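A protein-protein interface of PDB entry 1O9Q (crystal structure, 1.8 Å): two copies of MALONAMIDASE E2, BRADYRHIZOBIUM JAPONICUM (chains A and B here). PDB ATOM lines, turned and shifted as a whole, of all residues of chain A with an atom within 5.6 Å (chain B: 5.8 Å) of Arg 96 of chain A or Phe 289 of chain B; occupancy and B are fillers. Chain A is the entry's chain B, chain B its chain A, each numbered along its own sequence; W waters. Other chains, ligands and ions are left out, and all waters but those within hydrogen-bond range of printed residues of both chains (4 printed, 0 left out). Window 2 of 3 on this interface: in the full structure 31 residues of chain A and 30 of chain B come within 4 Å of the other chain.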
ATOM      1  N   GLN A  49       8.569 -25.203  34.956  1.00  0.00           N
ATOM      2  CA  GLN A  49       8.019 -24.003  34.316  1.00  0.00           C
ATOM      3  C   GLN A  49       6.496 -24.167  34.423  1.00  0.00           C
ATOM      4  O   GLN A  49       6.006 -25.279  34.621  1.00  0.00           O
ATOM      5  CB  GLN A  49       8.464 -23.925  32.851  1.00  0.00           C
ATOM      6  CG  GLN A  49       9.974 -23.742  32.663  1.00  0.00           C
ATOM      7  CD  GLN A  49      10.327 -23.206  31.283  1.00  0.00           C
ATOM      8  OE1 GLN A  49       9.927 -22.100  30.922  1.00  0.00           O
ATOM      9  NE2 GLN A  49      11.070 -23.991  30.505  1.00  0.00           N
ATOM     10  N   GLY A  52       3.651 -24.910  28.669  1.00  0.00           N
ATOM     11  CA  GLY A  52       4.353 -25.639  27.633  1.00  0.00           C
ATOM     12  C   GLY A  52       4.128 -27.131  27.740  1.00  0.00           C
ATOM     13  O   GLY A  52       3.871 -27.637  28.829  1.00  0.00           O
ATOM     14  N   VAL A  91      19.021 -26.982  23.525  1.00  0.00           N
ATOM     15  CA  VAL A  91      18.659 -26.777  24.929  1.00  0.00           C
ATOM     16  C   VAL A  91      17.506 -25.762  24.951  1.00  0.00           C
ATOM     17  O   VAL A  91      16.533 -25.922  25.685  1.00  0.00           O
ATOM     18  CB  VAL A  91      19.842 -26.219  25.744  1.00  0.00           C
ATOM     19  CG1 VAL A  91      19.363 -25.783  27.123  1.00  0.00           C
ATOM     20  CG2 VAL A  91      20.929 -27.284  25.868  1.00  0.00           C
ATOM     21  N   MET A  92      17.625 -24.717  24.138  1.00  0.00           N
ATOM     22  CA  MET A  92      16.569 -23.705  24.062  1.00  0.00           C
ATOM     23  C   MET A  92      15.272 -24.327  23.516  1.00  0.00           C
ATOM     24  O   MET A  92      14.183 -23.890  23.875  1.00  0.00           O
ATOM     25  CB  MET A  92      17.015 -22.545  23.167  1.00  0.00           C
ATOM     26  CG  MET A  92      18.036 -21.603  23.811  1.00  0.00           C
ATOM     27  SD  MET A  92      17.480 -20.921  25.402  1.00  0.00           S
ATOM     28  CE  MET A  92      15.961 -20.114  24.935  1.00  0.00           C
ATOM     29  N   MET A  93      15.386 -25.332  22.646  1.00  0.00           N
ATOM     30  CA  MET A  93      14.173 -25.993  22.111  1.00  0.00           C
ATOM     31  C   MET A  93      13.416 -26.623  23.289  1.00  0.00           C
ATOM     32  O   MET A  93      12.189 -26.574  23.354  1.00  0.00           O
ATOM     33  CB  MET A  93      14.553 -27.089  21.110  1.00  0.00           C
ATOM     34  CG  MET A  93      15.116 -26.594  19.781  1.00  0.00           C
ATOM     35  SD  MET A  93      15.535 -27.996  18.698  1.00  0.00           S
ATOM     36  CE  MET A  93      15.498 -27.214  17.073  1.00  0.00           C
ATOM     37  N   LEU A  94      14.164 -27.209  24.213  1.00  0.00           N
ATOM     38  CA  LEU A  94      13.560 -27.837  25.390  1.00  0.00           C
ATOM     39  C   LEU A  94      12.961 -26.768  26.319  1.00  0.00           C
ATOM     40  O   LEU A  94      11.804 -26.871  26.731  1.00  0.00           O
ATOM     41  CB  LEU A  94      14.635 -28.659  26.115  1.00  0.00           C
ATOM     42  CG  LEU A  94      15.106 -29.927  25.385  1.00  0.00           C
ATOM     43  CD1 LEU A  94      16.368 -30.484  26.041  1.00  0.00           C
ATOM     44  CD2 LEU A  94      13.990 -30.969  25.397  1.00  0.00           C
ATOM     45  N   LYS A  95      13.748 -25.741  26.629  1.00  0.00           N
ATOM     46  CA  LYS A  95      13.287 -24.668  27.514  1.00  0.00           C
ATOM     47  C   LYS A  95      12.048 -23.945  26.963  1.00  0.00           C
ATOM     48  O   LYS A  95      11.123 -23.638  27.710  1.00  0.00           O
ATOM     49  CB  LYS A  95      14.422 -23.661  27.730  1.00  0.00           C
ATOM     50  CG  LYS A  95      15.713 -24.270  28.248  1.00  0.00           C
ATOM     51  CD  LYS A  95      16.500 -23.288  29.113  1.00  0.00           C
ATOM     52  CE  LYS A  95      16.593 -21.899  28.501  1.00  0.00           C
ATOM     53  NZ  LYS A  95      17.394 -20.965  29.352  1.00  0.00           N
ATOM     54  N   ARG A  96      12.034 -23.675  25.662  1.00  0.00           N
ATOM     55  CA  ARG A  96      10.891 -22.983  25.065  1.00  0.00           C
ATOM     56  C   ARG A  96       9.619 -23.823  25.137  1.00  0.00           C
ATOM     57  O   ARG A  96       8.512 -23.290  25.093  1.00  0.00           O
ATOM     58  CB  ARG A  96      11.221 -22.617  23.618  1.00  0.00           C
ATOM     59  CG  ARG A  96      12.116 -21.385  23.496  1.00  0.00           C
ATOM     60  CD  ARG A  96      12.448 -21.092  22.051  1.00  0.00           C
ATOM     61  NE  ARG A  96      13.115 -19.803  21.886  1.00  0.00           N
ATOM     62  CZ  ARG A  96      13.248 -19.182  20.719  1.00  0.00           C
ATOM     63  NH1 ARG A  96      12.763 -19.733  19.611  1.00  0.00           N
ATOM     64  NH2 ARG A  96      13.853 -18.004  20.657  1.00  0.00           N
ATOM     65  N   ALA A  97       9.784 -25.135  25.261  1.00  0.00           N
ATOM     66  CA  ALA A  97       8.636 -26.036  25.349  1.00  0.00           C
ATOM     67  C   ALA A  97       8.149 -26.169  26.804  1.00  0.00           C
ATOM     68  O   ALA A  97       7.154 -26.844  27.073  1.00  0.00           O
ATOM     69  CB  ALA A  97       9.005 -27.407  24.782  1.00  0.00           C
ATOM     70  N   GLY A  98       8.860 -25.523  27.725  1.00  0.00           N
ATOM     71  CA  GLY A  98       8.488 -25.563  29.132  1.00  0.00           C
ATOM     72  C   GLY A  98       9.243 -26.573  29.981  1.00  0.00           C
ATOM     73  O   GLY A  98       8.916 -26.780  31.152  1.00  0.00           O
ATOM     74  N   ALA A  99      10.265 -27.197  29.405  1.00  0.00           N
ATOM     75  CA  ALA A  99      11.053 -28.205  30.137  1.00  0.00           C
ATOM     76  C   ALA A  99      12.026 -27.612  31.154  1.00  0.00           C
ATOM     77  O   ALA A  99      12.340 -26.418  31.126  1.00  0.00           O
ATOM     78  CB  ALA A  99      11.824 -29.077  29.153  1.00  0.00           C
ATOM     79  N   HIS B 282      16.155 -18.307  13.888  1.00  0.00           N
ATOM     80  CA  HIS B 282      15.376 -18.327  15.130  1.00  0.00           C
ATOM     81  C   HIS B 282      15.845 -19.443  16.061  1.00  0.00           C
ATOM     82  O   HIS B 282      15.815 -19.291  17.282  1.00  0.00           O
ATOM     83  CB  HIS B 282      13.894 -18.471  14.797  1.00  0.00           C
ATOM     84  CG  HIS B 282      13.193 -17.158  14.660  1.00  0.00           C
ATOM     85  ND1 HIS B 282      13.011 -16.306  15.728  1.00  0.00           N
ATOM     86  CD2 HIS B 282      12.685 -16.522  13.579  1.00  0.00           C
ATOM     87  CE1 HIS B 282      12.422 -15.201  15.309  1.00  0.00           C
ATOM     88  NE2 HIS B 282      12.215 -15.305  14.009  1.00  0.00           N
ATOM     89  N   ARG B 283      16.285 -20.558  15.479  1.00  0.00           N
ATOM     90  CA  ARG B 283      16.793 -21.685  16.280  1.00  0.00           C
ATOM     91  C   ARG B 283      18.213 -21.369  16.744  1.00  0.00           C
ATOM     92  O   ARG B 283      18.541 -21.524  17.919  1.00  0.00           O
ATOM     93  CB  ARG B 283      16.848 -22.965  15.436  1.00  0.00           C
ATOM     94  CG  ARG B 283      15.584 -23.824  15.413  1.00  0.00           C
ATOM     95  CD  ARG B 283      14.464 -23.175  14.633  1.00  0.00           C
ATOM     96  NE  ARG B 283      13.517 -22.502  15.512  1.00  0.00           N
ATOM     97  CZ  ARG B 283      12.517 -21.738  15.085  1.00  0.00           C
ATOM     98  NH1 ARG B 283      12.336 -21.543  13.787  1.00  0.00           N
ATOM     99  NH2 ARG B 283      11.692 -21.176  15.961  1.00  0.00           N
ATOM    100  N   LEU B 285      19.732 -18.538  17.084  1.00  0.00           N
ATOM    101  CA  LEU B 285      19.820 -17.407  18.021  1.00  0.00           C
ATOM    102  C   LEU B 285      18.693 -17.461  19.061  1.00  0.00           C
ATOM    103  O   LEU B 285      18.274 -16.432  19.593  1.00  0.00           O
ATOM    104  CB  LEU B 285      19.742 -16.103  17.220  1.00  0.00           C
ATOM    105  CG  LEU B 285      20.900 -15.846  16.253  1.00  0.00           C
ATOM    106  CD1 LEU B 285      20.623 -14.589  15.438  1.00  0.00           C
ATOM    107  CD2 LEU B 285      22.195 -15.711  17.036  1.00  0.00           C
ATOM    108  N   ALA B 286      18.221 -18.669  19.354  1.00  0.00           N
ATOM    109  CA  ALA B 286      17.125 -18.855  20.319  1.00  0.00           C
ATOM    110  C   ALA B 286      17.422 -18.233  21.686  1.00  0.00           C
ATOM    111  O   ALA B 286      16.593 -17.508  22.237  1.00  0.00           O
ATOM    112  CB  ALA B 286      16.819 -20.339  20.481  1.00  0.00           C
ATOM    113  N   TRP B 287      18.599 -18.518  22.230  1.00  0.00           N
ATOM    114  CA  TRP B 287      18.961 -17.975  23.537  1.00  0.00           C
ATOM    115  C   TRP B 287      18.926 -16.445  23.534  1.00  0.00           C
ATOM    116  O   TRP B 287      18.328 -15.834  24.420  1.00  0.00           O
ATOM    117  CB  TRP B 287      20.356 -18.465  23.922  1.00  0.00           C
ATOM    118  CG  TRP B 287      20.813 -17.944  25.247  1.00  0.00           C
ATOM    119  CD1 TRP B 287      20.457 -18.408  26.481  1.00  0.00           C
ATOM    120  CD2 TRP B 287      21.704 -16.848  25.472  1.00  0.00           C
ATOM    121  NE1 TRP B 287      21.074 -17.671  27.461  1.00  0.00           N
ATOM    122  CE2 TRP B 287      21.846 -16.706  26.871  1.00  0.00           C
ATOM    123  CE3 TRP B 287      22.400 -15.972  24.628  1.00  0.00           C
ATOM    124  CZ2 TRP B 287      22.655 -15.722  27.447  1.00  0.00           C
ATOM    125  CZ3 TRP B 287      23.206 -14.993  25.201  1.00  0.00           C
ATOM    126  CH2 TRP B 287      23.326 -14.879  26.598  1.00  0.00           C
ATOM    127  N   GLU B 288      19.563 -15.834  22.539  1.00  0.00           N
ATOM    128  CA  GLU B 288      19.590 -14.363  22.439  1.00  0.00           C
ATOM    129  C   GLU B 288      18.191 -13.745  22.299  1.00  0.00           C
ATOM    130  O   GLU B 288      17.859 -12.759  22.972  1.00  0.00           O
ATOM    131  CB  GLU B 288      20.457 -13.940  21.243  1.00  0.00           C
ATOM    132  CG  GLU B 288      21.951 -14.208  21.410  1.00  0.00           C
ATOM    133  CD  GLU B 288      22.368 -15.615  20.995  1.00  0.00           C
ATOM    134  OE1 GLU B 288      21.497 -16.501  20.844  1.00  0.00           O
ATOM    135  OE2 GLU B 288      23.581 -15.832  20.827  1.00  0.00           O
ATOM    136  N   PHE B 289      17.377 -14.332  21.428  1.00  0.00           N
ATOM    137  CA  PHE B 289      16.018 -13.829  21.180  1.00  0.00           C
ATOM    138  C   PHE B 289      15.088 -14.010  22.391  1.00  0.00           C
ATOM    139  O   PHE B 289      14.248 -13.155  22.667  1.00  0.00           O
ATOM    140  CB  PHE B 289      15.450 -14.562  19.962  1.00  0.00           C
ATOM    141  CG  PHE B 289      14.132 -14.017  19.481  1.00  0.00           C
ATOM    142  CD1 PHE B 289      14.086 -12.890  18.671  1.00  0.00           C
ATOM    143  CD2 PHE B 289      12.938 -14.631  19.844  1.00  0.00           C
ATOM    144  CE1 PHE B 289      12.868 -12.379  18.224  1.00  0.00           C
ATOM    145  CE2 PHE B 289      11.713 -14.128  19.405  1.00  0.00           C
ATOM    146  CZ  PHE B 289      11.680 -12.998  18.592  1.00  0.00           C
ATOM    147  N   SER B 290      15.250 -15.117  23.109  1.00  0.00           N
ATOM    148  CA  SER B 290      14.412 -15.402  24.282  1.00  0.00           C
ATOM    149  C   SER B 290      14.847 -14.702  25.577  1.00  0.00           C
ATOM    150  O   SER B 290      14.004 -14.257  26.350  1.00  0.00           O
ATOM    151  CB  SER B 290      14.384 -16.917  24.525  1.00  0.00           C
ATOM    152  OG  SER B 290      13.648 -17.593  23.517  1.00  0.00           O
ATOM    153  N   GLU B 291      16.155 -14.595  25.799  1.00  0.00           N
ATOM    154  CA  GLU B 291      16.682 -13.999  27.046  1.00  0.00           C
ATOM    155  C   GLU B 291      17.200 -12.557  26.957  1.00  0.00           C
ATOM    156  O   GLU B 291      17.293 -11.862  27.976  1.00  0.00           O
ATOM    157  CB  GLU B 291      17.822 -14.884  27.554  1.00  0.00           C
ATOM    158  CG  GLU B 291      17.561 -16.372  27.524  1.00  0.00           C
ATOM    159  CD  GLU B 291      16.620 -16.832  28.608  1.00  0.00           C
ATOM    160  OE1 GLU B 291      16.588 -18.053  28.876  1.00  0.00           O
ATOM    161  OE2 GLU B 291      15.909 -15.983  29.186  1.00  0.00           O
ATOM    162  N   HIS B 292      17.554 -12.118  25.756  1.00  0.00           N
ATOM    163  CA  HIS B 292      18.098 -10.768  25.576  1.00  0.00           C
ATOM    164  C   HIS B 292      17.520 -10.095  24.344  1.00  0.00           C
ATOM    165  O   HIS B 292      18.223  -9.376  23.630  1.00  0.00           O
ATOM    166  CB  HIS B 292      19.617 -10.897  25.462  1.00  0.00           C
ATOM    167  CG  HIS B 292      20.248 -11.545  26.653  1.00  0.00           C
ATOM    168  ND1 HIS B 292      20.574 -10.845  27.796  1.00  0.00           N
ATOM    169  CD2 HIS B 292      20.535 -12.844  26.914  1.00  0.00           C
ATOM    170  CE1 HIS B 292      21.031 -11.684  28.709  1.00  0.00           C
ATOM    171  NE2 HIS B 292      21.017 -12.903  28.199  1.00  0.00           N
ATOM    172  N   HIS B 293      16.233 -10.329  24.114  1.00  0.00           N
ATOM    173  CA  HIS B 293      15.524  -9.789  22.957  1.00  0.00           C
ATOM    174  C   HIS B 293      15.782  -8.314  22.684  1.00  0.00           C
ATOM    175  O   HIS B 293      16.208  -7.948  21.592  1.00  0.00           O
ATOM    176  CB  HIS B 293      14.024 -10.032  23.141  1.00  0.00           C
ATOM    177  CG  HIS B 293      13.192  -9.596  21.974  1.00  0.00           C
ATOM    178  ND1 HIS B 293      12.750  -8.300  21.813  1.00  0.00           N
ATOM    179  CD2 HIS B 293      12.748 -10.280  20.892  1.00  0.00           C
ATOM    180  CE1 HIS B 293      12.070  -8.204  20.685  1.00  0.00           C
ATOM    181  NE2 HIS B 293      12.055  -9.391  20.105  1.00  0.00           N
ATOM    182  N   ILE B 296      19.169  -7.188  21.255  1.00  0.00           N
ATOM    183  CA  ILE B 296      19.541  -7.534  19.882  1.00  0.00           C
ATOM    184  C   ILE B 296      19.427  -6.255  19.047  1.00  0.00           C
ATOM    185  O   ILE B 296      18.424  -5.541  19.135  1.00  0.00           O
ATOM    186  CB  ILE B 296      18.603  -8.610  19.298  1.00  0.00           C
ATOM    187  CG1 ILE B 296      18.734  -9.900  20.110  1.00  0.00           C
ATOM    188  CG2 ILE B 296      18.931  -8.846  17.818  1.00  0.00           C
ATOM    189  CD1 ILE B 296      17.790 -11.013  19.674  1.00  0.00           C
ATOM    190  N   ARG B 301      16.788  -7.548  15.148  1.00  0.00           N
ATOM    191  CA  ARG B 301      15.661  -7.792  16.053  1.00  0.00           C
ATOM    192  C   ARG B 301      14.351  -7.713  15.271  1.00  0.00           C
ATOM    193  O   ARG B 301      13.432  -8.503  15.496  1.00  0.00           O
ATOM    194  CB  ARG B 301      15.669  -6.755  17.181  1.00  0.00           C
ATOM    195  CG  ARG B 301      14.667  -7.070  18.287  1.00  0.00           C
ATOM    196  CD  ARG B 301      14.860  -6.195  19.521  1.00  0.00           C
ATOM    197  NE  ARG B 301      14.370  -4.832  19.339  1.00  0.00           N
ATOM    198  CZ  ARG B 301      15.128  -3.744  19.425  1.00  0.00           C
ATOM    199  NH1 ARG B 301      16.425  -3.850  19.688  1.00  0.00           N
ATOM    200  NH2 ARG B 301      14.586  -2.546  19.259  1.00  0.00           N
ATOM    201  N   LEU B 304      13.922 -10.811  12.918  1.00  0.00           N
ATOM    202  CA  LEU B 304      13.570 -11.993  13.722  1.00  0.00           C
ATOM    203  C   LEU B 304      12.098 -11.891  14.167  1.00  0.00           C
ATOM    204  O   LEU B 304      11.341 -12.853  14.081  1.00  0.00           O
ATOM    205  CB  LEU B 304      14.505 -12.075  14.933  1.00  0.00           C
ATOM    206  CG  LEU B 304      15.950 -12.503  14.635  1.00  0.00           C
ATOM    207  CD1 LEU B 304      16.850 -12.216  15.829  1.00  0.00           C
ATOM    208  CD2 LEU B 304      15.973 -13.984  14.291  1.00  0.00           C
ATOM    209  N   ASP B 305      11.702 -10.713  14.627  1.00  0.00           N
ATOM    210  CA  ASP B 305      10.320 -10.491  15.068  1.00  0.00           C
ATOM    211  C   ASP B 305       9.303 -10.759  13.951  1.00  0.00           C
ATOM    212  O   ASP B 305       8.243 -11.329  14.194  1.00  0.00           O
ATOM    213  CB  ASP B 305      10.184  -9.048  15.555  1.00  0.00           C
ATOM    214  CG  ASP B 305      10.692  -8.857  16.968  1.00  0.00           C
ATOM    215  OD1 ASP B 305      10.862  -7.691  17.384  1.00  0.00           O
ATOM    216  OD2 ASP B 305      10.912  -9.866  17.670  1.00  0.00           O
ATOM    217  N   VAL B 308       8.980 -14.918  13.321  1.00  0.00           N
ATOM    218  CA  VAL B 308       8.748 -15.919  14.373  1.00  0.00           C
ATOM    219  C   VAL B 308       7.719 -16.973  13.934  1.00  0.00           C
ATOM    220  O   VAL B 308       7.711 -18.091  14.448  1.00  0.00           O
ATOM    221  CB  VAL B 308       8.231 -15.274  15.685  1.00  0.00           C
ATOM    222  CG1 VAL B 308       9.248 -14.284  16.215  1.00  0.00           C
ATOM    223  CG2 VAL B 308       6.895 -14.598  15.445  1.00  0.00           C
HETATM  224  O   HOH W   1      10.805 -21.929  18.787  1.00  0.00           O
HETATM  225  O   HOH W   2      14.444 -17.116  18.195  1.00  0.00           O
HETATM  226  O   HOH W   3      11.249 -17.805  17.756  1.00  0.00           O
HETATM  227  O   HOH W   4      13.822 -22.817  18.679  1.00  0.00           O
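The guanidinium group (NH2) of Arg 96 of chain A lies within hydrogen-bond range of the backbone carbonyl oxygen (O) of Ala 286 of chain B (3.2 Å). OG of Ser 290 of chain B lies within hydrogen-bond range of NE of Arg 96 of chain A (2.8 Å). OE1 of Glu 291 of chain B lies within salt-bridge range of NZ of Lys 95 of chain A (3.1 Å).
NE2 of His 282 of chain B sits at hydrogen-bond distance from O of Leu 304 of chain B, 2.6 Å away. A ring nitrogen (NE2) of His 282 of chain B sits at hydrogen-bond distance from the backbone NH (N) of Val 308 of chain B (3.3 Å). The backbone carbonyl oxygen (O) of Ala 286 of chain B is in hydrogen-bond range of the side-chain hydroxyl (OG) of Ser 290 of chain B, 3.2 Å away. The side-chain amide nitrogen (NE2) of Gln 49 of chain A sits at hydrogen-bond distance from the backbone carbonyl oxygen (O) of Lys 95 of chain A (2.8 Å).
Ala 286 of chain B touches Met 92 of chain A. CG of Met 92 of chain A touches N of Trp 287 of chain B, at 3.5 Å. Ser 290 of chain B touches Met 92 of chain A (CB to CE, 3.6 Å). Met 93 of chain A touches Arg 283 of chain B (CE to CG, 3.8 Å). O of His 282 of chain B touches NH1 of Arg 96 of chain A, 3.9 Å away. Arg 96 of chain A touches Phe 289 of chain B (NH2 to CD2, 3.6 Å).
Printed residues of chain B within 4 Å of Met 93 of chain A: Arg 283. Leu 94 of chain A touches none of the printed residues of chain B. Of the printed residues of chain B, Arg 96 of chain A touches His 282 (3.9 Å), Ala 286 (3.2 Å), Phe 289 (3.6 Å) and Ser 290 (2.8 Å). Printed residues of chain A within 4 Å of His 282 of chain B: Arg 96 (3.9 Å). Printed residues of chain A within 4 Å of Trp 287 of chain B: Met 92. Phe 289 of chain B touches just one residue of chain A: Arg 96 (3.6 Å). The nearest printed residue of chain B that does not touch Met 93 of chain A is Ala 286 of chain B (5.6 Å).
Hydrophobic or aromatic side chains of chain A that line the printed part of chain B: Met 92 and Met 93.
No position is printed for both chains.
Water W2 lies within hydrogen-bond range of the guanidinium group of Arg 96 of chain A (2.7 Å) and the backbone carbonyl oxygen of His 282 of chain B (2.7 Å). Water W1 lies within hydrogen-bond range of the guanidinium group of Arg 96 of chain A (3.1 Å) and the guanidinium group of Arg 283 of chain B (3.1 Å). Water W3 bridges the guanidinium group (NH1) of Arg 96 of chain A and a ring nitrogen (ND1) of His 282 of chain B. Water W4 lies within hydrogen-bond range of NE of Arg 283 of chain B (3.2 Å) and NH1 of Arg 96 of chain A (3.4 Å).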
